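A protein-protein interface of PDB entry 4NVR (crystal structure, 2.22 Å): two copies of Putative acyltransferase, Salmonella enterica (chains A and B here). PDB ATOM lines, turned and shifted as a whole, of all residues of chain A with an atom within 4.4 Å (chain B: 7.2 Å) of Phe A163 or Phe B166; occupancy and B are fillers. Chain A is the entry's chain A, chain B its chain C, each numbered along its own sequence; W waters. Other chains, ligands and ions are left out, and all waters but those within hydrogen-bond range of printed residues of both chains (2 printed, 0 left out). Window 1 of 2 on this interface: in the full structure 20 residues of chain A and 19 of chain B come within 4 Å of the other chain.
O of Thr A160 sits at hydrogen-bond distance from NE2 of Gln B170.
O of Lys A156 sits at hydrogen-bond distance from OG1 of Thr A160, 2.6 Å away.
The side-chain hydroxyl of Thr B154 is in hydrogen-bond range of the backbone carbonyl oxygen of Tyr B151.
The backbone carbonyl oxygen (O) of Trp B165 sits at hydrogen-bond distance from the side-chain hydroxyl (OH) of Tyr B151.
The backbone carbonyl oxygen (O) of Phe B166 sits at hydrogen-bond distance from the side-chain amide nitrogen (NE2) of Gln B170, at 3.0 Å.
Thr B154 touches Lys A156 (CB to N, 3.6 Å).
Ala B159 touches Ala A159 (CB to CB, 3.9 Å).
OG1 of Thr A160 touches CD1 of Ile B169 (3.97 Å).
CB of Phe A163 touches O of Phe B166, at 3.5 Å.
Gln B170 touches Phe A163.
Phe A163 touches Leu B174.
Phe A166 touches Ala B159 (CD1 to CB, 3.5 Å).
Phe B163 touches Phe A166 (CB to O, 3.7 Å).
CE2 of Phe B163 touches CD1 of Phe A167, 3.7 Å away.
Phe A167 touches Met B178.
Of chain B, only Phe B166, Gln B170 and Leu B174 come within 4 Å of Phe A163.
Phe B166 touches just these residues of chain A: Lys A156 (3.8 Å), Ala A159 (3.4 Å), Thr A160 (3.8 Å) and Phe A163 (3.5 Å).
Printed residues of chain B within 4 Å of Thr A160: Phe B166 (3.8 Å), Ile B169 (3.97 Å) and Gln B170 (2.8 Å).
Printed residues of chain A within 4 Å of Phe B163: Phe A166 (3.7 Å) and Phe A167 (3.7 Å).
Of the printed residues of chain A, Leu B174 touches Phe A163 (3.8 Å).
The nearest residue of chain B that does not touch Phe A163 is Phe B167 (4.2 Å).
Printed residues of chain B that touch a printed residue of chain A: Tyr B151, Thr B154, Ala B159, Thr B160, Phe B163, Phe B166, Ile B169, Gln B170, Leu B174 and Met B178.
Of the 10 printed residues of chain A, 6 touch a printed residue of chain B.
Hydrophobic or aromatic side chains of chain A within 4 Å of the printed part of chain B: Ala A159, Phe A163, Phe A166 and Phe A167.
Among the printed residues, no Asp or Glu carboxylate lies within 4 Å of a Lys or Arg side-chain nitrogen of the other chain.
Ala B159 touches its own counterpart, Ala A159.
Ala A159 touches Phe B166, and with the chains exchanged Phe A166 touches Ala B159.
Phe A163 touches Phe B166, and with the chains exchanged Phe A166 touches Phe B163.
Phe A167 touches Phe B163, but with the chains exchanged Phe A163 does not touch Phe B167 (4.2 Å).
Water W2 lies within hydrogen-bond range of OE1 of Gln B170 (2.6 Å) and O of Thr A160 (3.0 Å).
Water W1 lies within hydrogen-bond range of N of Lys A156 (2.7 Å) and O of Tyr B151 (3.1 Å).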
ATOM      1  N   LYS A 156     -12.083  17.425  -7.903  1.00  0.00           N
ATOM      2  CA  LYS A 156     -12.431  18.578  -7.084  1.00  0.00           C
ATOM      3  C   LYS A 156     -11.186  19.397  -6.681  1.00  0.00           C
ATOM      4  O   LYS A 156     -11.155  20.609  -6.810  1.00  0.00           O
ATOM      5  CB  LYS A 156     -13.137  18.096  -5.844  1.00  0.00           C
ATOM      6  CG  LYS A 156     -13.763  19.203  -5.035  1.00  0.00           C
ATOM      7  CD  LYS A 156     -14.568  18.578  -3.918  1.00  0.00           C
ATOM      8  CE  LYS A 156     -15.328  19.627  -3.118  1.00  0.00           C
ATOM      9  NZ  LYS A 156     -14.417  20.539  -2.389  1.00  0.00           N
ATOM     10  N   ALA A 159      -9.330  21.160  -9.808  1.00  0.00           N
ATOM     11  CA  ALA A 159     -10.119  22.318 -10.260  1.00  0.00           C
ATOM     12  C   ALA A 159     -10.096  23.473  -9.252  1.00  0.00           C
ATOM     13  O   ALA A 159     -10.275  24.629  -9.618  1.00  0.00           O
ATOM     14  CB  ALA A 159     -11.555  21.906 -10.579  1.00  0.00           C
ATOM     15  N   THR A 160      -9.847  23.157  -7.986  1.00  0.00           N
ATOM     16  CA  THR A 160      -9.794  24.203  -6.962  1.00  0.00           C
ATOM     17  C   THR A 160      -8.434  24.917  -6.969  1.00  0.00           C
ATOM     18  O   THR A 160      -8.350  26.136  -7.045  1.00  0.00           O
ATOM     19  CB  THR A 160     -10.067  23.649  -5.550  1.00  0.00           C
ATOM     20  OG1 THR A 160     -11.291  22.890  -5.551  1.00  0.00           O
ATOM     21  CG2 THR A 160     -10.182  24.792  -4.571  1.00  0.00           C
ATOM     22  N   ARG A 161      -7.386  24.127  -6.900  1.00  0.00           N
ATOM     23  CA  ARG A 161      -6.000  24.623  -6.870  1.00  0.00           C
ATOM     24  C   ARG A 161      -5.562  25.260  -8.193  1.00  0.00           C
ATOM     25  O   ARG A 161      -4.783  26.182  -8.197  1.00  0.00           O
ATOM     26  CB  ARG A 161      -5.094  23.457  -6.483  1.00  0.00           C
ATOM     27  CG  ARG A 161      -5.490  22.820  -5.146  1.00  0.00           C
ATOM     28  CD  ARG A 161      -4.794  23.489  -3.979  1.00  0.00           C
ATOM     29  NE  ARG A 161      -3.405  23.017  -3.910  1.00  0.00           N
ATOM     30  CZ  ARG A 161      -2.476  23.461  -3.067  1.00  0.00           C
ATOM     31  NH1 ARG A 161      -1.253  22.939  -3.107  1.00  0.00           N
ATOM     32  NH2 ARG A 161      -2.753  24.427  -2.191  1.00  0.00           N
ATOM     33  N   TYR A 162      -6.074  24.766  -9.312  1.00  0.00           N
ATOM     34  CA  TYR A 162      -5.774  25.319 -10.641  1.00  0.00           C
ATOM     35  C   TYR A 162      -7.024  25.940 -11.272  1.00  0.00           C
ATOM     36  O   TYR A 162      -7.309  25.726 -12.444  1.00  0.00           O
ATOM     37  CB  TYR A 162      -5.213  24.223 -11.578  1.00  0.00           C
ATOM     38  CG  TYR A 162      -3.800  23.798 -11.238  1.00  0.00           C
ATOM     39  CD1 TYR A 162      -2.711  24.527 -11.693  1.00  0.00           C
ATOM     40  CD2 TYR A 162      -3.554  22.681 -10.468  1.00  0.00           C
ATOM     41  CE1 TYR A 162      -1.413  24.161 -11.394  1.00  0.00           C
ATOM     42  CE2 TYR A 162      -2.261  22.307 -10.158  1.00  0.00           C
ATOM     43  CZ  TYR A 162      -1.200  23.059 -10.621  1.00  0.00           C
ATOM     44  OH  TYR A 162       0.075  22.697 -10.315  1.00  0.00           O
ATOM     45  N   PHE A 163      -7.746  26.771 -10.533  1.00  0.00           N
ATOM     46  CA  PHE A 163      -8.999  27.267 -11.081  1.00  0.00           C
ATOM     47  C   PHE A 163      -8.846  28.086 -12.344  1.00  0.00           C
ATOM     48  O   PHE A 163      -9.739  28.090 -13.147  1.00  0.00           O
ATOM     49  CB  PHE A 163      -9.839  28.007 -10.053  1.00  0.00           C
ATOM     50  CG  PHE A 163      -9.409  29.398  -9.821  1.00  0.00           C
ATOM     51  CD1 PHE A 163      -8.396  29.671  -8.946  1.00  0.00           C
ATOM     52  CD2 PHE A 163     -10.056  30.437 -10.466  1.00  0.00           C
ATOM     53  CE1 PHE A 163      -7.991  30.976  -8.735  1.00  0.00           C
ATOM     54  CE2 PHE A 163      -9.673  31.737 -10.254  1.00  0.00           C
ATOM     55  CZ  PHE A 163      -8.638  32.009  -9.378  1.00  0.00           C
ATOM     56  N   TRP A 164      -7.721  28.758 -12.545  1.00  0.00           N
ATOM     57  CA  TRP A 164      -7.522  29.520 -13.808  1.00  0.00           C
ATOM     58  C   TRP A 164      -7.593  28.617 -15.057  1.00  0.00           C
ATOM     59  O   TRP A 164      -7.938  29.078 -16.142  1.00  0.00           O
ATOM     60  CB  TRP A 164      -6.205  30.261 -13.801  1.00  0.00           C
ATOM     61  CG  TRP A 164      -6.041  31.185 -12.690  1.00  0.00           C
ATOM     62  CD1 TRP A 164      -5.200  31.034 -11.612  1.00  0.00           C
ATOM     63  CD2 TRP A 164      -6.737  32.414 -12.478  1.00  0.00           C
ATOM     64  NE1 TRP A 164      -5.325  32.092 -10.761  1.00  0.00           N
ATOM     65  CE2 TRP A 164      -6.255  32.961 -11.264  1.00  0.00           C
ATOM     66  CE3 TRP A 164      -7.705  33.118 -13.198  1.00  0.00           C
ATOM     67  CZ2 TRP A 164      -6.709  34.182 -10.757  1.00  0.00           C
ATOM     68  CZ3 TRP A 164      -8.163  34.341 -12.692  1.00  0.00           C
ATOM     69  CH2 TRP A 164      -7.671  34.854 -11.477  1.00  0.00           C
ATOM     70  N   TRP A 165      -7.267  27.335 -14.899  1.00  0.00           N
ATOM     71  CA  TRP A 165      -7.306  26.378 -16.013  1.00  0.00           C
ATOM     72  C   TRP A 165      -8.710  26.106 -16.515  1.00  0.00           C
ATOM     73  O   TRP A 165      -8.888  25.497 -17.591  1.00  0.00           O
ATOM     74  CB  TRP A 165      -6.632  25.075 -15.605  1.00  0.00           C
ATOM     75  CG  TRP A 165      -5.139  25.166 -15.620  1.00  0.00           C
ATOM     76  CD1 TRP A 165      -4.357  26.124 -15.017  1.00  0.00           C
ATOM     77  CD2 TRP A 165      -4.225  24.227 -16.223  1.00  0.00           C
ATOM     78  NE1 TRP A 165      -3.046  25.846 -15.224  1.00  0.00           N
ATOM     79  CE2 TRP A 165      -2.920  24.707 -15.972  1.00  0.00           C
ATOM     80  CE3 TRP A 165      -4.388  23.045 -16.960  1.00  0.00           C
ATOM     81  CZ2 TRP A 165      -1.776  24.043 -16.417  1.00  0.00           C
ATOM     82  CZ3 TRP A 165      -3.241  22.388 -17.424  1.00  0.00           C
ATOM     83  CH2 TRP A 165      -1.959  22.881 -17.139  1.00  0.00           C
ATOM     84  N   PHE A 166      -9.695  26.542 -15.724  1.00  0.00           N
ATOM     85  CA  PHE A 166     -11.117  26.443 -16.063  1.00  0.00           C
ATOM     86  C   PHE A 166     -11.756  27.822 -16.267  1.00  0.00           C
ATOM     87  O   PHE A 166     -12.835  27.950 -16.865  1.00  0.00           O
ATOM     88  CB  PHE A 166     -11.849  25.599 -15.004  1.00  0.00           C
ATOM     89  CG  PHE A 166     -11.294  24.216 -14.905  1.00  0.00           C
ATOM     90  CD1 PHE A 166     -11.610  23.261 -15.879  1.00  0.00           C
ATOM     91  CD2 PHE A 166     -10.388  23.887 -13.921  1.00  0.00           C
ATOM     92  CE1 PHE A 166     -11.042  21.999 -15.848  1.00  0.00           C
ATOM     93  CE2 PHE A 166      -9.839  22.628 -13.876  1.00  0.00           C
ATOM     94  CZ  PHE A 166     -10.154  21.682 -14.846  1.00  0.00           C
ATOM     95  N   PHE A 167     -11.081  28.860 -15.802  1.00  0.00           N
ATOM     96  CA  PHE A 167     -11.568  30.220 -15.978  1.00  0.00           C
ATOM     97  C   PHE A 167     -10.986  30.858 -17.247  1.00  0.00           C
ATOM     98  O   PHE A 167     -11.690  31.499 -18.022  1.00  0.00           O
ATOM     99  CB  PHE A 167     -11.184  31.046 -14.761  1.00  0.00           C
ATOM    100  CG  PHE A 167     -11.715  32.445 -14.781  1.00  0.00           C
ATOM    101  CD1 PHE A 167     -12.986  32.718 -14.332  1.00  0.00           C
ATOM    102  CD2 PHE A 167     -10.921  33.482 -15.218  1.00  0.00           C
ATOM    103  CE1 PHE A 167     -13.475  34.017 -14.344  1.00  0.00           C
ATOM    104  CE2 PHE A 167     -11.382  34.776 -15.232  1.00  0.00           C
ATOM    105  CZ  PHE A 167     -12.662  35.049 -14.803  1.00  0.00           C
ATOM    106  N   MET B 150     -22.239  15.942  -7.433  1.00  0.00           N
ATOM    107  CA  MET B 150     -21.661  16.872  -8.402  1.00  0.00           C
ATOM    108  C   MET B 150     -20.186  17.079  -8.175  1.00  0.00           C
ATOM    109  O   MET B 150     -19.381  16.985  -9.120  1.00  0.00           O
ATOM    110  CB  MET B 150     -22.473  18.171  -8.399  1.00  0.00           C
ATOM    111  CG  MET B 150     -23.733  17.833  -9.189  1.00  0.00           C
ATOM    112  SD  MET B 150     -25.008  19.308  -9.400  1.00  0.00           S
ATOM    113  CE  MET B 150     -23.863  20.171 -10.755  1.00  0.00           C
ATOM    114  N   TYR B 151     -19.809  17.383  -6.940  1.00  0.00           N
ATOM    115  CA  TYR B 151     -18.397  17.526  -6.628  1.00  0.00           C
ATOM    116  C   TYR B 151     -17.619  16.196  -6.834  1.00  0.00           C
ATOM    117  O   TYR B 151     -16.500  16.212  -7.337  1.00  0.00           O
ATOM    118  CB  TYR B 151     -18.182  18.107  -5.218  1.00  0.00           C
ATOM    119  CG  TYR B 151     -18.119  19.637  -5.182  1.00  0.00           C
ATOM    120  CD1 TYR B 151     -17.234  20.323  -5.996  1.00  0.00           C
ATOM    121  CD2 TYR B 151     -18.897  20.392  -4.306  1.00  0.00           C
ATOM    122  CE1 TYR B 151     -17.145  21.705  -5.967  1.00  0.00           C
ATOM    123  CE2 TYR B 151     -18.800  21.782  -4.274  1.00  0.00           C
ATOM    124  CZ  TYR B 151     -17.917  22.426  -5.116  1.00  0.00           C
ATOM    125  OH  TYR B 151     -17.778  23.794  -5.124  1.00  0.00           O
ATOM    126  N   THR B 154     -16.599  15.445 -10.351  1.00  0.00           N
ATOM    127  CA  THR B 154     -15.860  16.538 -10.947  1.00  0.00           C
ATOM    128  C   THR B 154     -14.877  16.055 -12.013  1.00  0.00           C
ATOM    129  O   THR B 154     -13.971  15.267 -11.723  1.00  0.00           O
ATOM    130  CB  THR B 154     -15.093  17.406  -9.914  1.00  0.00           C
ATOM    131  OG1 THR B 154     -16.028  18.105  -9.077  1.00  0.00           O
ATOM    132  CG2 THR B 154     -14.230  18.456 -10.645  1.00  0.00           C
ATOM    133  N   ASP B 155     -15.116  16.494 -13.246  1.00  0.00           N
ATOM    134  CA  ASP B 155     -14.198  16.228 -14.357  1.00  0.00           C
ATOM    135  C   ASP B 155     -14.016  17.497 -15.182  1.00  0.00           C
ATOM    136  O   ASP B 155     -14.571  18.567 -14.856  1.00  0.00           O
ATOM    137  CB  ASP B 155     -14.619  15.012 -15.227  1.00  0.00           C
ATOM    138  CG  ASP B 155     -15.993  15.179 -15.907  1.00  0.00           C
ATOM    139  OD1 ASP B 155     -16.657  16.235 -15.751  1.00  0.00           O
ATOM    140  OD2 ASP B 155     -16.410  14.201 -16.581  1.00  0.00           O
ATOM    141  N   PHE B 158     -17.135  19.211 -16.466  1.00  0.00           N
ATOM    142  CA  PHE B 158     -17.877  19.792 -15.353  1.00  0.00           C
ATOM    143  C   PHE B 158     -17.262  21.069 -14.843  1.00  0.00           C
ATOM    144  O   PHE B 158     -17.947  22.071 -14.656  1.00  0.00           O
ATOM    145  CB  PHE B 158     -17.993  18.846 -14.171  1.00  0.00           C
ATOM    146  CG  PHE B 158     -18.731  19.464 -13.014  1.00  0.00           C
ATOM    147  CD1 PHE B 158     -20.059  19.792 -13.149  1.00  0.00           C
ATOM    148  CD2 PHE B 158     -18.085  19.763 -11.835  1.00  0.00           C
ATOM    149  CE1 PHE B 158     -20.750  20.377 -12.117  1.00  0.00           C
ATOM    150  CE2 PHE B 158     -18.759  20.349 -10.794  1.00  0.00           C
ATOM    151  CZ  PHE B 158     -20.100  20.663 -10.928  1.00  0.00           C
ATOM    152  N   ALA B 159     -15.964  21.031 -14.587  1.00  0.00           N
ATOM    153  CA  ALA B 159     -15.282  22.204 -14.067  1.00  0.00           C
ATOM    154  C   ALA B 159     -15.291  23.314 -15.103  1.00  0.00           C
ATOM    155  O   ALA B 159     -15.203  24.493 -14.753  1.00  0.00           O
ATOM    156  CB  ALA B 159     -13.869  21.857 -13.663  1.00  0.00           C
ATOM    157  N   THR B 160     -15.395  22.932 -16.377  1.00  0.00           N
ATOM    158  CA  THR B 160     -15.468  23.894 -17.478  1.00  0.00           C
ATOM    159  C   THR B 160     -16.883  24.513 -17.580  1.00  0.00           C
ATOM    160  O   THR B 160     -17.036  25.727 -17.660  1.00  0.00           O
ATOM    161  CB  THR B 160     -15.144  23.210 -18.833  1.00  0.00           C
ATOM    162  OG1 THR B 160     -13.830  22.649 -18.799  1.00  0.00           O
ATOM    163  CG2 THR B 160     -15.258  24.216 -20.007  1.00  0.00           C
ATOM    164  N   TYR B 162     -19.455  24.316 -15.302  1.00  0.00           N
ATOM    165  CA  TYR B 162     -19.821  24.903 -14.003  1.00  0.00           C
ATOM    166  C   TYR B 162     -18.555  25.479 -13.296  1.00  0.00           C
ATOM    167  O   TYR B 162     -18.330  25.263 -12.087  1.00  0.00           O
ATOM    168  CB  TYR B 162     -20.533  23.824 -13.157  1.00  0.00           C
ATOM    169  CG  TYR B 162     -22.063  23.900 -13.154  1.00  0.00           C
ATOM    170  CD1 TYR B 162     -22.780  24.119 -14.325  1.00  0.00           C
ATOM    171  CD2 TYR B 162     -22.788  23.712 -11.971  1.00  0.00           C
ATOM    172  CE1 TYR B 162     -24.166  24.191 -14.322  1.00  0.00           C
ATOM    173  CE2 TYR B 162     -24.188  23.782 -11.959  1.00  0.00           C
ATOM    174  CZ  TYR B 162     -24.871  24.017 -13.144  1.00  0.00           C
ATOM    175  OH  TYR B 162     -26.247  24.085 -13.176  1.00  0.00           O
ATOM    176  N   PHE B 163     -17.746  26.234 -14.062  1.00  0.00           N
ATOM    177  CA  PHE B 163     -16.488  26.772 -13.546  1.00  0.00           C
ATOM    178  C   PHE B 163     -16.717  27.603 -12.281  1.00  0.00           C
ATOM    179  O   PHE B 163     -15.879  27.578 -11.342  1.00  0.00           O
ATOM    180  CB  PHE B 163     -15.725  27.567 -14.613  1.00  0.00           C
ATOM    181  CG  PHE B 163     -16.308  28.924 -14.885  1.00  0.00           C
ATOM    182  CD1 PHE B 163     -17.360  29.078 -15.779  1.00  0.00           C
ATOM    183  CD2 PHE B 163     -15.827  30.036 -14.217  1.00  0.00           C
ATOM    184  CE1 PHE B 163     -17.929  30.325 -16.014  1.00  0.00           C
ATOM    185  CE2 PHE B 163     -16.383  31.279 -14.442  1.00  0.00           C
ATOM    186  CZ  PHE B 163     -17.441  31.424 -15.346  1.00  0.00           C
ATOM    187  N   TRP B 164     -17.858  28.290 -12.197  1.00  0.00           N
ATOM    188  CA  TRP B 164     -18.124  29.068 -10.970  1.00  0.00           C
ATOM    189  C   TRP B 164     -18.092  28.207  -9.677  1.00  0.00           C
ATOM    190  O   TRP B 164     -17.884  28.741  -8.596  1.00  0.00           O
ATOM    191  CB  TRP B 164     -19.385  29.929 -11.077  1.00  0.00           C
ATOM    192  CG  TRP B 164     -20.690  29.209 -11.236  1.00  0.00           C
ATOM    193  CD1 TRP B 164     -21.577  28.876 -10.237  1.00  0.00           C
ATOM    194  CD2 TRP B 164     -21.293  28.781 -12.467  1.00  0.00           C
ATOM    195  NE1 TRP B 164     -22.698  28.255 -10.783  1.00  0.00           N
ATOM    196  CE2 TRP B 164     -22.540  28.173 -12.140  1.00  0.00           C
ATOM    197  CE3 TRP B 164     -20.904  28.846 -13.807  1.00  0.00           C
ATOM    198  CZ2 TRP B 164     -23.387  27.633 -13.104  1.00  0.00           C
ATOM    199  CZ3 TRP B 164     -21.740  28.299 -14.765  1.00  0.00           C
ATOM    200  CH2 TRP B 164     -22.981  27.697 -14.401  1.00  0.00           C
ATOM    201  N   TRP B 165     -18.246  26.885  -9.775  1.00  0.00           N
ATOM    202  CA  TRP B 165     -18.137  26.046  -8.581  1.00  0.00           C
ATOM    203  C   TRP B 165     -16.670  25.955  -8.111  1.00  0.00           C
ATOM    204  O   TRP B 165     -16.356  25.350  -7.077  1.00  0.00           O
ATOM    205  CB  TRP B 165     -18.701  24.647  -8.849  1.00  0.00           C
ATOM    206  CG  TRP B 165     -20.235  24.536  -8.782  1.00  0.00           C
ATOM    207  CD1 TRP B 165     -21.139  25.316  -9.427  1.00  0.00           C
ATOM    208  CD2 TRP B 165     -21.002  23.537  -8.089  1.00  0.00           C
ATOM    209  NE1 TRP B 165     -22.425  24.897  -9.138  1.00  0.00           N
ATOM    210  CE2 TRP B 165     -22.353  23.786  -8.347  1.00  0.00           C
ATOM    211  CE3 TRP B 165     -20.672  22.458  -7.279  1.00  0.00           C
ATOM    212  CZ2 TRP B 165     -23.363  23.022  -7.792  1.00  0.00           C
ATOM    213  CZ3 TRP B 165     -21.656  21.703  -6.751  1.00  0.00           C
ATOM    214  CH2 TRP B 165     -22.988  21.982  -6.995  1.00  0.00           C
ATOM    215  N   PHE B 166     -15.767  26.563  -8.876  1.00  0.00           N
ATOM    216  CA  PHE B 166     -14.356  26.550  -8.512  1.00  0.00           C
ATOM    217  C   PHE B 166     -13.787  27.952  -8.387  1.00  0.00           C
ATOM    218  O   PHE B 166     -12.676  28.129  -7.934  1.00  0.00           O
ATOM    219  CB  PHE B 166     -13.605  25.681  -9.510  1.00  0.00           C
ATOM    220  CG  PHE B 166     -14.087  24.266  -9.493  1.00  0.00           C
ATOM    221  CD1 PHE B 166     -13.742  23.429  -8.446  1.00  0.00           C
ATOM    222  CD2 PHE B 166     -14.937  23.791 -10.467  1.00  0.00           C
ATOM    223  CE1 PHE B 166     -14.211  22.135  -8.383  1.00  0.00           C
ATOM    224  CE2 PHE B 166     -15.431  22.494 -10.399  1.00  0.00           C
ATOM    225  CZ  PHE B 166     -15.077  21.672  -9.358  1.00  0.00           C
ATOM    226  N   PHE B 167     -14.597  28.938  -8.747  1.00  0.00           N
ATOM    227  CA  PHE B 167     -14.216  30.326  -8.719  1.00  0.00           C
ATOM    228  C   PHE B 167     -14.780  31.011  -7.483  1.00  0.00           C
ATOM    229  O   PHE B 167     -14.032  31.706  -6.750  1.00  0.00           O
ATOM    230  CB  PHE B 167     -14.690  30.997 -10.003  1.00  0.00           C
ATOM    231  CG  PHE B 167     -14.713  32.482  -9.934  1.00  0.00           C
ATOM    232  CD1 PHE B 167     -13.575  33.204 -10.134  1.00  0.00           C
ATOM    233  CD2 PHE B 167     -15.895  33.160  -9.664  1.00  0.00           C
ATOM    234  CE1 PHE B 167     -13.590  34.581 -10.074  1.00  0.00           C
ATOM    235  CE2 PHE B 167     -15.923  34.545  -9.608  1.00  0.00           C
ATOM    236  CZ  PHE B 167     -14.769  35.257  -9.816  1.00  0.00           C
ATOM    237  N   LEU B 168     -16.078  30.801  -7.222  1.00  0.00           N
ATOM    238  CA  LEU B 168     -16.717  31.423  -6.054  1.00  0.00           C
ATOM    239  C   LEU B 168     -16.203  30.829  -4.765  1.00  0.00           C
ATOM    240  O   LEU B 168     -16.381  31.423  -3.697  1.00  0.00           O
ATOM    241  CB  LEU B 168     -18.241  31.265  -6.097  1.00  0.00           C
ATOM    242  CG  LEU B 168     -18.959  31.887  -7.301  1.00  0.00           C
ATOM    243  CD1 LEU B 168     -20.393  31.398  -7.394  1.00  0.00           C
ATOM    244  CD2 LEU B 168     -18.910  33.408  -7.260  1.00  0.00           C
ATOM    245  N   ILE B 169     -15.559  29.661  -4.840  1.00  0.00           N
ATOM    246  CA  ILE B 169     -15.044  29.056  -3.633  1.00  0.00           C
ATOM    247  C   ILE B 169     -13.598  29.428  -3.349  1.00  0.00           C
ATOM    248  O   ILE B 169     -13.079  28.986  -2.341  1.00  0.00           O
ATOM    249  CB  ILE B 169     -15.173  27.526  -3.592  1.00  0.00           C
ATOM    250  CG1 ILE B 169     -14.208  26.867  -4.597  1.00  0.00           C
ATOM    251  CG2 ILE B 169     -16.622  27.099  -3.783  1.00  0.00           C
ATOM    252  CD1 ILE B 169     -14.170  25.370  -4.417  1.00  0.00           C
ATOM    253  N   GLN B 170     -12.956  30.235  -4.203  1.00  0.00           N
ATOM    254  CA  GLN B 170     -11.609  30.685  -3.905  1.00  0.00           C
ATOM    255  C   GLN B 170     -11.632  31.514  -2.609  1.00  0.00           C
ATOM    256  O   GLN B 170     -12.655  32.142  -2.278  1.00  0.00           O
ATOM    257  CB  GLN B 170     -11.007  31.469  -5.064  1.00  0.00           C
ATOM    258  CG  GLN B 170     -10.664  30.603  -6.283  1.00  0.00           C
ATOM    259  CD  GLN B 170      -9.730  29.437  -5.942  1.00  0.00           C
ATOM    260  OE1 GLN B 170      -8.665  29.621  -5.340  1.00  0.00           O
ATOM    261  NE2 GLN B 170     -10.130  28.221  -6.337  1.00  0.00           N
ATOM    262  N   PRO B 171     -10.515  31.508  -1.850  1.00  0.00           N
ATOM    263  CA  PRO B 171     -10.482  32.226  -0.557  1.00  0.00           C
ATOM    264  C   PRO B 171     -10.830  33.718  -0.621  1.00  0.00           C
ATOM    265  O   PRO B 171     -10.562  34.387  -1.611  1.00  0.00           O
ATOM    266  CB  PRO B 171      -9.029  32.047  -0.073  1.00  0.00           C
ATOM    267  CG  PRO B 171      -8.443  30.946  -0.894  1.00  0.00           C
ATOM    268  CD  PRO B 171      -9.185  30.975  -2.215  1.00  0.00           C
ATOM    269  N   LEU B 174     -10.970  37.105  -3.069  1.00  0.00           N
ATOM    270  CA  LEU B 174     -10.765  37.004  -4.519  1.00  0.00           C
ATOM    271  C   LEU B 174     -12.029  37.067  -5.359  1.00  0.00           C
ATOM    272  O   LEU B 174     -12.199  37.981  -6.170  1.00  0.00           O
ATOM    273  CB  LEU B 174      -9.928  35.753  -4.852  1.00  0.00           C
ATOM    274  CG  LEU B 174      -9.505  35.506  -6.315  1.00  0.00           C
ATOM    275  CD1 LEU B 174      -8.892  36.737  -6.976  1.00  0.00           C
ATOM    276  CD2 LEU B 174      -8.508  34.358  -6.373  1.00  0.00           C
ATOM    277  N   MET B 178     -13.364  40.410  -7.633  1.00  0.00           N
ATOM    278  CA  MET B 178     -13.571  40.315  -9.068  1.00  0.00           C
ATOM    279  C   MET B 178     -14.991  40.667  -9.475  1.00  0.00           C
ATOM    280  O   MET B 178     -15.206  41.380 -10.460  1.00  0.00           O
ATOM    281  CB  MET B 178     -13.148  38.922  -9.522  1.00  0.00           C
ATOM    282  CG  MET B 178     -11.618  38.881  -9.597  1.00  0.00           C
ATOM    283  SD  MET B 178     -10.978  37.078 -10.099  1.00  0.00           S
ATOM    284  CE  MET B 178     -11.925  36.911 -11.827  1.00  0.00           C
ATOM    285  N   TYR B 226     -21.292  29.165  -1.513  1.00  0.00           N
ATOM    286  CA  TYR B 226     -20.622  28.185  -2.361  1.00  0.00           C
ATOM    287  C   TYR B 226     -19.479  27.520  -1.611  1.00  0.00           C
ATOM    288  O   TYR B 226     -19.211  26.331  -1.803  1.00  0.00           O
ATOM    289  CB  TYR B 226     -20.138  28.829  -3.660  1.00  0.00           C
ATOM    290  CG  TYR B 226     -21.216  28.913  -4.709  1.00  0.00           C
ATOM    291  CD1 TYR B 226     -22.211  29.886  -4.648  1.00  0.00           C
ATOM    292  CD2 TYR B 226     -21.247  28.014  -5.767  1.00  0.00           C
ATOM    293  CE1 TYR B 226     -23.219  29.946  -5.620  1.00  0.00           C
ATOM    294  CE2 TYR B 226     -22.242  28.072  -6.733  1.00  0.00           C
ATOM    295  CZ  TYR B 226     -23.224  29.040  -6.661  1.00  0.00           C
ATOM    296  OH  TYR B 226     -24.214  29.093  -7.619  1.00  0.00           O
HETATM  297  O   HOH W   1     -13.563  15.230  -7.332  1.00  0.00           O
HETATM  298  O   HOH W   2      -6.777  27.853  -5.130  1.00  0.00           O
